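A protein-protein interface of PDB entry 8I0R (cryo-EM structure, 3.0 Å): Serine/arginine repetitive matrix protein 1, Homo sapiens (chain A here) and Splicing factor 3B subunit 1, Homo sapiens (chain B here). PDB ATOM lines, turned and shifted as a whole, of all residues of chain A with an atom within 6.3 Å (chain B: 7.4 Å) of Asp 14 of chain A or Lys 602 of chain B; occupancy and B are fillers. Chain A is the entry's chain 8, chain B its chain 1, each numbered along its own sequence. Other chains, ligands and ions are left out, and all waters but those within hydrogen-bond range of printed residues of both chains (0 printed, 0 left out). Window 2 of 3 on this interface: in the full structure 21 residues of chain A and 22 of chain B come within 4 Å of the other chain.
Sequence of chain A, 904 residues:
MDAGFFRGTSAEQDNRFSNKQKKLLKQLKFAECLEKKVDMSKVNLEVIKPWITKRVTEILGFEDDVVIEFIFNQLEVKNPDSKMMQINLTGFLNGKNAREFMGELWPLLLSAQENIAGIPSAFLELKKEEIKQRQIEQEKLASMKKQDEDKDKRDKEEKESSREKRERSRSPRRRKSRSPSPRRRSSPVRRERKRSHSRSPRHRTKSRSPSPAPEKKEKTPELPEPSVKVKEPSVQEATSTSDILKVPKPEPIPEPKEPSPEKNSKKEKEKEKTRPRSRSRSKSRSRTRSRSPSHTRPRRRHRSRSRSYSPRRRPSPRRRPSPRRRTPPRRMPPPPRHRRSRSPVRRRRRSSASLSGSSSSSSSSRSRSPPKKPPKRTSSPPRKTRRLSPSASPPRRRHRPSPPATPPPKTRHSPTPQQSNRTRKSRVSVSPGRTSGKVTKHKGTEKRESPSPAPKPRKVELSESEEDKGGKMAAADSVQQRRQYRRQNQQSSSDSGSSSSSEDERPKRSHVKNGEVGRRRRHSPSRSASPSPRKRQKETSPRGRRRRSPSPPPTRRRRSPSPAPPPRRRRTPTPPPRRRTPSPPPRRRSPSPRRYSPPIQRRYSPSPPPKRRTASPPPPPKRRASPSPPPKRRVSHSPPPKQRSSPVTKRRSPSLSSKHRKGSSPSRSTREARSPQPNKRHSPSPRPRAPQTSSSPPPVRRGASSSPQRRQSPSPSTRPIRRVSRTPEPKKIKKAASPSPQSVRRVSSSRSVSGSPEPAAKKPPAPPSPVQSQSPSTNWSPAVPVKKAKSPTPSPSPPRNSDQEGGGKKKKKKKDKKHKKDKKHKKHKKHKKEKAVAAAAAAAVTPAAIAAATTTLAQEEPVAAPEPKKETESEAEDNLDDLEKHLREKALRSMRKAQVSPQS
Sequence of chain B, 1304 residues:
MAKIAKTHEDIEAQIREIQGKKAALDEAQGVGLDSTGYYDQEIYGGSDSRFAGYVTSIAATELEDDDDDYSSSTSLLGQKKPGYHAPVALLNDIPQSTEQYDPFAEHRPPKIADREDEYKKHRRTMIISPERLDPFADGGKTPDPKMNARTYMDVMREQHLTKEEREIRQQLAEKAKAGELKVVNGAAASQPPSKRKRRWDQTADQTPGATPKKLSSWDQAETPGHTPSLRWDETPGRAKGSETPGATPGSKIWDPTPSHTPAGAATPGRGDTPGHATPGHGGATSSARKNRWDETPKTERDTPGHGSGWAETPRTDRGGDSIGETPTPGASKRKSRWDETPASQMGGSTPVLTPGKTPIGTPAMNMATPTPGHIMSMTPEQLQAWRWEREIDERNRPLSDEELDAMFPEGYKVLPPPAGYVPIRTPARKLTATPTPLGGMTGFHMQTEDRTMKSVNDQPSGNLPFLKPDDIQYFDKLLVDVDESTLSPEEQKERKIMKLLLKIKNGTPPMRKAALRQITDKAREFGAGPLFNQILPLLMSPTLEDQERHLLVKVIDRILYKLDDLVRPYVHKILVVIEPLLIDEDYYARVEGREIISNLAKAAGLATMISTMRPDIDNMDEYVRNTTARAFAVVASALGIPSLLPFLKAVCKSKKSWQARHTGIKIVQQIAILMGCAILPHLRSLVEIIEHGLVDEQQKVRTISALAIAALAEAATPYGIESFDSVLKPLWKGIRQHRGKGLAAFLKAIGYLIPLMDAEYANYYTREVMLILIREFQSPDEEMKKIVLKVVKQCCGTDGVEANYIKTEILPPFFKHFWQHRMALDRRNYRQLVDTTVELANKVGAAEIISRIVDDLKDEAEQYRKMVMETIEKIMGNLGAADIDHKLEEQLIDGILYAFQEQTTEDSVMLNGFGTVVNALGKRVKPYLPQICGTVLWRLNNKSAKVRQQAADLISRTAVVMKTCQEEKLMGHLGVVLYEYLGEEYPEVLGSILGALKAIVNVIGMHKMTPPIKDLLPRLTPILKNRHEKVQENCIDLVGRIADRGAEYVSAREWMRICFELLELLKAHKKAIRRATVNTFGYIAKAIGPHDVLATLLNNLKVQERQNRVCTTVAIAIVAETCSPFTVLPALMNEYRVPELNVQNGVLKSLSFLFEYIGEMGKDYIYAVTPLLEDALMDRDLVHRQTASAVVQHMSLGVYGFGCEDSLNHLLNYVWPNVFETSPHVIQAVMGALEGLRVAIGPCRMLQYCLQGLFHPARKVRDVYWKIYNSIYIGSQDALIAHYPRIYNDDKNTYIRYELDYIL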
ATOM      1  N   GLU A  12      11.121  -4.406  30.793  1.00  0.00           N
ATOM      2  CA  GLU A  12      10.791  -3.349  31.740  1.00  0.00           C
ATOM      3  C   GLU A  12       9.292  -3.224  31.899  1.00  0.00           C
ATOM      4  O   GLU A  12       8.776  -3.187  33.010  1.00  0.00           O
ATOM      5  CB  GLU A  12      11.378  -2.011  31.289  1.00  0.00           C
ATOM      6  CG  GLU A  12      11.296  -1.757  29.788  1.00  0.00           C
ATOM      7  CD  GLU A  12      11.298  -0.284  29.446  1.00  0.00           C
ATOM      8  OE1 GLU A  12      10.706   0.088  28.415  1.00  0.00           O
ATOM      9  OE2 GLU A  12      11.892   0.499  30.211  1.00  0.00           O
ATOM     10  N   GLN A  13       8.595  -3.142  30.772  1.00  0.00           N
ATOM     11  CA  GLN A  13       7.146  -3.015  30.771  1.00  0.00           C
ATOM     12  C   GLN A  13       6.474  -4.097  29.933  1.00  0.00           C
ATOM     13  O   GLN A  13       5.296  -4.400  30.149  1.00  0.00           O
ATOM     14  CB  GLN A  13       6.761  -1.621  30.272  1.00  0.00           C
ATOM     15  CG  GLN A  13       7.424  -0.509  31.069  1.00  0.00           C
ATOM     16  CD  GLN A  13       7.677   0.738  30.250  1.00  0.00           C
ATOM     17  OE1 GLN A  13       7.890   0.668  29.041  1.00  0.00           O
ATOM     18  NE2 GLN A  13       7.667   1.890  30.907  1.00  0.00           N
ATOM     19  N   ASP A  14       7.205  -4.705  29.000  1.00  0.00           N
ATOM     20  CA  ASP A  14       6.652  -5.665  28.055  1.00  0.00           C
ATOM     21  C   ASP A  14       6.851  -7.088  28.560  1.00  0.00           C
ATOM     22  O   ASP A  14       7.847  -7.394  29.224  1.00  0.00           O
ATOM     23  CB  ASP A  14       7.300  -5.508  26.674  1.00  0.00           C
ATOM     24  CG  ASP A  14       6.717  -6.460  25.622  1.00  0.00           C
ATOM     25  OD1 ASP A  14       5.854  -7.304  25.949  1.00  0.00           O
ATOM     26  OD2 ASP A  14       7.123  -6.351  24.447  1.00  0.00           O
ATOM     27  N   ASN A  15       5.895  -7.953  28.223  1.00  0.00           N
ATOM     28  CA  ASN A  15       5.912  -9.363  28.588  1.00  0.00           C
ATOM     29  C   ASN A  15       6.095 -10.253  27.366  1.00  0.00           C
ATOM     30  O   ASN A  15       6.536 -11.397  27.481  1.00  0.00           O
ATOM     31  CB  ASN A  15       4.620  -9.734  29.314  1.00  0.00           C
ATOM     32  CG  ASN A  15       3.388  -9.485  28.467  1.00  0.00           C
ATOM     33  OD1 ASN A  15       3.488  -9.064  27.317  1.00  0.00           O
ATOM     34  ND2 ASN A  15       2.220  -9.747  29.034  1.00  0.00           N
ATOM     35  N   ARG A  16       5.762  -9.725  26.190  1.00  0.00           N
ATOM     36  CA  ARG A  16       5.690 -10.508  24.966  1.00  0.00           C
ATOM     37  C   ARG A  16       7.034 -10.688  24.277  1.00  0.00           C
ATOM     38  O   ARG A  16       7.069 -11.193  23.151  1.00  0.00           O
ATOM     39  CB  ARG A  16       4.707  -9.853  23.989  1.00  0.00           C
ATOM     40  CG  ARG A  16       3.302 -10.444  24.024  1.00  0.00           C
ATOM     41  CD  ARG A  16       2.398  -9.796  22.981  1.00  0.00           C
ATOM     42  NE  ARG A  16       2.972  -8.556  22.456  1.00  0.00           N
ATOM     43  CZ  ARG A  16       2.563  -7.331  22.780  1.00  0.00           C
ATOM     44  NH1 ARG A  16       1.572  -7.153  23.646  1.00  0.00           N
ATOM     45  NH2 ARG A  16       3.159  -6.274  22.245  1.00  0.00           N
ATOM     46  N   PHE A  17       8.130 -10.277  24.909  1.00  0.00           N
ATOM     47  CA  PHE A  17       9.473 -10.529  24.406  1.00  0.00           C
ATOM     48  C   PHE A  17      10.306 -11.222  25.474  1.00  0.00           C
ATOM     49  O   PHE A  17      10.108 -11.001  26.672  1.00  0.00           O
ATOM     50  CB  PHE A  17      10.149  -9.232  23.963  1.00  0.00           C
ATOM     51  CG  PHE A  17       9.951  -8.909  22.508  1.00  0.00           C
ATOM     52  CD1 PHE A  17       9.748  -9.917  21.587  1.00  0.00           C
ATOM     53  CD2 PHE A  17       9.973  -7.600  22.065  1.00  0.00           C
ATOM     54  CE1 PHE A  17       9.569  -9.620  20.261  1.00  0.00           C
ATOM     55  CE2 PHE A  17       9.792  -7.305  20.742  1.00  0.00           C
ATOM     56  CZ  PHE A  17       9.594  -8.313  19.838  1.00  0.00           C
ATOM     57  N   SER A  18      11.234 -12.065  25.033  1.00  0.00           N
ATOM     58  CA  SER A  18      12.053 -12.873  25.925  1.00  0.00           C
ATOM     59  C   SER A  18      13.425 -12.241  26.144  1.00  0.00           C
ATOM     60  O   SER A  18      13.867 -11.396  25.362  1.00  0.00           O
ATOM     61  CB  SER A  18      12.211 -14.278  25.356  1.00  0.00           C
ATOM     62  OG  SER A  18      12.390 -14.238  23.951  1.00  0.00           O
ATOM     63  N   LYS A  20      16.895 -12.157  25.553  1.00  0.00           N
ATOM     64  CA  LYS A  20      17.768 -12.794  24.581  1.00  0.00           C
ATOM     65  C   LYS A  20      19.125 -13.118  25.170  1.00  0.00           C
ATOM     66  O   LYS A  20      19.733 -14.121  24.773  1.00  0.00           O
ATOM     67  CB  LYS A  20      17.908 -11.909  23.348  1.00  0.00           C
ATOM     68  CG  LYS A  20      16.571 -11.569  22.691  1.00  0.00           C
ATOM     69  CD  LYS A  20      15.630 -12.771  22.650  1.00  0.00           C
ATOM     70  CE  LYS A  20      14.284 -12.411  22.043  1.00  0.00           C
ATOM     71  NZ  LYS A  20      13.763 -11.112  22.540  1.00  0.00           N
ATOM     72  N   TYR B 561       7.533  -8.733  15.189  1.00  0.00           N
ATOM     73  CA  TYR B 561       7.111  -9.335  16.443  1.00  0.00           C
ATOM     74  C   TYR B 561       6.968 -10.842  16.343  1.00  0.00           C
ATOM     75  O   TYR B 561       7.173 -11.534  17.341  1.00  0.00           O
ATOM     76  CB  TYR B 561       5.792  -8.715  16.917  1.00  0.00           C
ATOM     77  CG  TYR B 561       5.020  -9.583  17.880  1.00  0.00           C
ATOM     78  CD1 TYR B 561       5.215  -9.470  19.246  1.00  0.00           C
ATOM     79  CD2 TYR B 561       4.071 -10.491  17.426  1.00  0.00           C
ATOM     80  CE1 TYR B 561       4.516 -10.263  20.132  1.00  0.00           C
ATOM     81  CE2 TYR B 561       3.366 -11.285  18.303  1.00  0.00           C
ATOM     82  CZ  TYR B 561       3.588 -11.166  19.657  1.00  0.00           C
ATOM     83  OH  TYR B 561       2.883 -11.950  20.541  1.00  0.00           O
ATOM     84  N   ASP B 564      11.195 -13.452  16.033  1.00  0.00           N
ATOM     85  CA  ASP B 564      11.853 -12.768  17.135  1.00  0.00           C
ATOM     86  C   ASP B 564      13.357 -12.692  16.919  1.00  0.00           C
ATOM     87  O   ASP B 564      13.915 -11.606  16.774  1.00  0.00           O
ATOM     88  CB  ASP B 564      11.539 -13.478  18.458  1.00  0.00           C
ATOM     89  CG  ASP B 564      11.614 -14.991  18.338  1.00  0.00           C
ATOM     90  OD1 ASP B 564      11.837 -15.486  17.214  1.00  0.00           O
ATOM     91  OD2 ASP B 564      11.467 -15.685  19.368  1.00  0.00           O
ATOM     92  N   GLU B 595       9.133   3.239  17.982  1.00  0.00           N
ATOM     93  CA  GLU B 595       8.567   2.027  18.556  1.00  0.00           C
ATOM     94  C   GLU B 595       9.118   0.775  17.883  1.00  0.00           C
ATOM     95  O   GLU B 595       9.451  -0.210  18.556  1.00  0.00           O
ATOM     96  CB  GLU B 595       7.051   2.081  18.456  1.00  0.00           C
ATOM     97  CG  GLU B 595       6.331   1.536  19.667  1.00  0.00           C
ATOM     98  CD  GLU B 595       6.232   0.034  19.652  1.00  0.00           C
ATOM     99  OE1 GLU B 595       5.614  -0.535  20.575  1.00  0.00           O
ATOM    100  OE2 GLU B 595       6.743  -0.579  18.695  1.00  0.00           O
ATOM    101  N   ILE B 596       9.244   0.785  16.559  1.00  0.00           N
ATOM    102  CA  ILE B 596       9.751  -0.432  15.944  1.00  0.00           C
ATOM    103  C   ILE B 596      11.242  -0.568  16.182  1.00  0.00           C
ATOM    104  O   ILE B 596      11.750  -1.687  16.246  1.00  0.00           O
ATOM    105  CB  ILE B 596       9.426  -0.544  14.444  1.00  0.00           C
ATOM    106  CG1 ILE B 596      10.550   0.002  13.593  1.00  0.00           C
ATOM    107  CG2 ILE B 596       8.152   0.149  14.100  1.00  0.00           C
ATOM    108  CD1 ILE B 596      10.441  -0.447  12.199  1.00  0.00           C
ATOM    109  N   ILE B 597      11.981   0.530  16.328  1.00  0.00           N
ATOM    110  CA  ILE B 597      13.389   0.366  16.669  1.00  0.00           C
ATOM    111  C   ILE B 597      13.523  -0.205  18.068  1.00  0.00           C
ATOM    112  O   ILE B 597      14.419  -1.007  18.343  1.00  0.00           O
ATOM    113  CB  ILE B 597      14.149   1.690  16.526  1.00  0.00           C
ATOM    114  CG1 ILE B 597      14.266   2.070  15.063  1.00  0.00           C
ATOM    115  CG2 ILE B 597      15.519   1.562  17.112  1.00  0.00           C
ATOM    116  CD1 ILE B 597      15.223   3.183  14.821  1.00  0.00           C
ATOM    117  N   SER B 598      12.620   0.173  18.967  1.00  0.00           N
ATOM    118  CA  SER B 598      12.607  -0.442  20.286  1.00  0.00           C
ATOM    119  C   SER B 598      12.375  -1.944  20.196  1.00  0.00           C
ATOM    120  O   SER B 598      13.103  -2.734  20.808  1.00  0.00           O
ATOM    121  CB  SER B 598      11.539   0.214  21.148  1.00  0.00           C
ATOM    122  OG  SER B 598      10.955  -0.739  22.011  1.00  0.00           O
ATOM    123  N   ASN B 599      11.346  -2.360  19.456  1.00  0.00           N
ATOM    124  CA  ASN B 599      11.082  -3.792  19.337  1.00  0.00           C
ATOM    125  C   ASN B 599      12.235  -4.513  18.664  1.00  0.00           C
ATOM    126  O   ASN B 599      12.540  -5.656  19.002  1.00  0.00           O
ATOM    127  CB  ASN B 599       9.799  -4.045  18.565  1.00  0.00           C
ATOM    128  CG  ASN B 599       8.582  -3.558  19.288  1.00  0.00           C
ATOM    129  OD1 ASN B 599       8.597  -3.368  20.497  1.00  0.00           O
ATOM    130  ND2 ASN B 599       7.504  -3.374  18.552  1.00  0.00           N
ATOM    131  N   LEU B 600      12.881  -3.870  17.698  1.00  0.00           N
ATOM    132  CA  LEU B 600      14.065  -4.447  17.075  1.00  0.00           C
ATOM    133  C   LEU B 600      15.164  -4.672  18.097  1.00  0.00           C
ATOM    134  O   LEU B 600      15.787  -5.738  18.125  1.00  0.00           O
ATOM    135  CB  LEU B 600      14.558  -3.531  15.967  1.00  0.00           C
ATOM    136  CG  LEU B 600      15.655  -4.059  15.061  1.00  0.00           C
ATOM    137  CD1 LEU B 600      15.132  -5.209  14.269  1.00  0.00           C
ATOM    138  CD2 LEU B 600      16.090  -2.964  14.141  1.00  0.00           C
ATOM    139  N   ALA B 601      15.433  -3.669  18.929  1.00  0.00           N
ATOM    140  CA  ALA B 601      16.472  -3.802  19.941  1.00  0.00           C
ATOM    141  C   ALA B 601      16.152  -4.923  20.908  1.00  0.00           C
ATOM    142  O   ALA B 601      17.044  -5.663  21.322  1.00  0.00           O
ATOM    143  CB  ALA B 601      16.638  -2.488  20.691  1.00  0.00           C
ATOM    144  N   LYS B 602      14.888  -5.055  21.296  1.00  0.00           N
ATOM    145  CA  LYS B 602      14.530  -6.153  22.186  1.00  0.00           C
ATOM    146  C   LYS B 602      14.667  -7.502  21.504  1.00  0.00           C
ATOM    147  O   LYS B 602      15.123  -8.461  22.129  1.00  0.00           O
ATOM    148  CB  LYS B 602      13.110  -5.997  22.706  1.00  0.00           C
ATOM    149  CG  LYS B 602      12.906  -4.839  23.617  1.00  0.00           C
ATOM    150  CD  LYS B 602      11.447  -4.617  23.823  1.00  0.00           C
ATOM    151  CE  LYS B 602      11.211  -3.733  25.004  1.00  0.00           C
ATOM    152  NZ  LYS B 602      10.383  -4.440  26.005  1.00  0.00           N
ATOM    153  N   ALA B 603      14.279  -7.604  20.237  1.00  0.00           N
ATOM    154  CA  ALA B 603      14.301  -8.895  19.570  1.00  0.00           C
ATOM    155  C   ALA B 603      15.731  -9.320  19.286  1.00  0.00           C
ATOM    156  O   ALA B 603      16.198 -10.331  19.811  1.00  0.00           O
ATOM    157  CB  ALA B 603      13.494  -8.841  18.278  1.00  0.00           C
ATOM    158  N   ALA B 604      16.443  -8.556  18.473  1.00  0.00           N
ATOM    159  CA  ALA B 604      17.863  -8.805  18.318  1.00  0.00           C
ATOM    160  C   ALA B 604      18.611  -8.140  19.461  1.00  0.00           C
ATOM    161  O   ALA B 604      18.652  -6.915  19.560  1.00  0.00           O
ATOM    162  CB  ALA B 604      18.347  -8.277  16.980  1.00  0.00           C
ATOM    163  N   GLY B 605      19.210  -8.955  20.325  1.00  0.00           N
ATOM    164  CA  GLY B 605      19.703  -8.461  21.595  1.00  0.00           C
ATOM    165  C   GLY B 605      20.840  -7.470  21.452  1.00  0.00           C
ATOM    166  O   GLY B 605      21.178  -7.018  20.363  1.00  0.00           O
ATOM    167  N   LEU B 606      21.441  -7.128  22.593  1.00  0.00           N
ATOM    168  CA  LEU B 606      22.420  -6.047  22.642  1.00  0.00           C
ATOM    169  C   LEU B 606      23.557  -6.254  21.655  1.00  0.00           C
ATOM    170  O   LEU B 606      23.804  -5.410  20.791  1.00  0.00           O
ATOM    171  CB  LEU B 606      22.978  -5.898  24.052  1.00  0.00           C
ATOM    172  CG  LEU B 606      24.123  -4.890  24.081  1.00  0.00           C
ATOM    173  CD1 LEU B 606      23.592  -3.497  23.854  1.00  0.00           C
ATOM    174  CD2 LEU B 606      24.867  -4.963  25.388  1.00  0.00           C
ATOM    175  N   MET B 609      22.997  -5.369  18.122  1.00  0.00           N
ATOM    176  CA  MET B 609      22.812  -3.951  17.839  1.00  0.00           C
ATOM    177  C   MET B 609      24.135  -3.213  17.900  1.00  0.00           C
ATOM    178  O   MET B 609      24.460  -2.416  17.014  1.00  0.00           O
ATOM    179  CB  MET B 609      21.818  -3.334  18.817  1.00  0.00           C
ATOM    180  CG  MET B 609      20.477  -4.016  18.873  1.00  0.00           C
ATOM    181  SD  MET B 609      19.576  -3.952  17.323  1.00  0.00           S
ATOM    182  CE  MET B 609      19.881  -2.271  16.818  1.00  0.00           C
ATOM    183  N   VAL B 635      17.759   2.393  21.474  1.00  0.00           N
ATOM    184  CA  VAL B 635      18.081   1.057  21.973  1.00  0.00           C
ATOM    185  C   VAL B 635      18.604   1.147  23.393  1.00  0.00           C
ATOM    186  O   VAL B 635      18.459   0.208  24.177  1.00  0.00           O
ATOM    187  CB  VAL B 635      19.062   0.295  21.055  1.00  0.00           C
ATOM    188  CG1 VAL B 635      19.301   1.021  19.782  1.00  0.00           C
ATOM    189  CG2 VAL B 635      20.369   0.036  21.755  1.00  0.00           C
ATOM    190  N   SER B 637      17.296   3.261  25.634  1.00  0.00           N
ATOM    191  CA  SER B 637      16.058   3.250  26.398  1.00  0.00           C
ATOM    192  C   SER B 637      15.479   1.850  26.501  1.00  0.00           C
ATOM    193  O   SER B 637      14.939   1.471  27.542  1.00  0.00           O
ATOM    194  CB  SER B 637      15.043   4.181  25.757  1.00  0.00           C
ATOM    195  OG  SER B 637      13.746   3.644  25.901  1.00  0.00           O
ATOM    196  N   ALA B 638      15.574   1.068  25.430  1.00  0.00           N
ATOM    197  CA  ALA B 638      14.894  -0.223  25.411  1.00  0.00           C
ATOM    198  C   ALA B 638      15.654  -1.273  26.211  1.00  0.00           C
ATOM    199  O   ALA B 638      15.045  -2.172  26.796  1.00  0.00           O
ATOM    200  CB  ALA B 638      14.692  -0.692  23.974  1.00  0.00           C
ATOM    201  N   LEU B 639      16.984  -1.195  26.231  1.00  0.00           N
ATOM    202  CA  LEU B 639      17.804  -2.237  26.835  1.00  0.00           C
ATOM    203  C   LEU B 639      18.398  -1.854  28.181  1.00  0.00           C
ATOM    204  O   LEU B 639      18.823  -2.742  28.925  1.00  0.00           O
ATOM    205  CB  LEU B 639      18.936  -2.623  25.887  1.00  0.00           C
ATOM    206  CG  LEU B 639      18.479  -3.400  24.661  1.00  0.00           C
ATOM    207  CD1 LEU B 639      19.656  -3.982  23.920  1.00  0.00           C
ATOM    208  CD2 LEU B 639      17.535  -4.486  25.102  1.00  0.00           C
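The side-chain carboxylate (OE2) of Glu 595 of chain B lies within hydrogen-bond range of the side-chain amide nitrogen (ND2) of Asn 599 of chain B (2.9 Å). The side-chain amide oxygen of Asn 15 of chain A lies close to the side-chain carboxylate of Asp 14 of chain A. The side-chain carboxylate (OD1) of Asp 14 of chain A lies within hydrogen-bond range of the backbone NH (N) of Arg 16 of chain A (2.4 Å). The backbone carbonyl oxygen (O) of Ser 18 of chain A lies within hydrogen-bond range of the side-chain amino group (NZ) of Lys 20 of chain A.
Of the 19 printed residues of chain B, 4 touch a printed residue of chain A. Of the 8 printed residues of chain A, 4 touch a printed residue of chain B. Hydrophobic or aromatic side chains of chain A within 4 Å of the printed part of chain B: Phe 17. Among the printed residues, 6 pairs touch across the chains.
Among the printed residues, merely in contact across the chains: Lys 20 of chain A with Ala 603 of chain B (3.2 Å), Arg 16 of chain A with Tyr 561 of chain B (3.3 Å), Asp 14 of chain A with Lys 602 of chain B (3.3 Å), Phe 17 of chain A with Lys 602 of chain B (3.6 Å) and Phe 17 of chain A with Asn 599 of chain B (3.6 Å).
Of chain B, only Lys 602 (3.3 Å) comes within 4 Å of Asp 14 of chain A. Of chain A, only Asp 14, Phe 17 and Lys 20 come within 4 Å of Lys 602 of chain B. Printed residues of chain B within 4 Å of Phe 17 of chain A: Asn 599 (3.6 Å) and Lys 602 (3.6 Å). Of the printed residues of chain B, Arg 16 of chain A touches Tyr 561. Of the printed residues of chain A, Ala 603 of chain B touches Lys 20. Of the printed residues of chain B, Lys 20 of chain A touches Lys 602 (3.0 Å) and Ala 603 (3.2 Å). Printed residues of chain A within 4 Å of Asn 599 of chain B: Phe 17. Ile 597 of chain B touches none of the printed residues of chain A.
NZ of Lys 20 of chain A sits at hydrogen-bond distance from O of Lys 602 of chain B.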
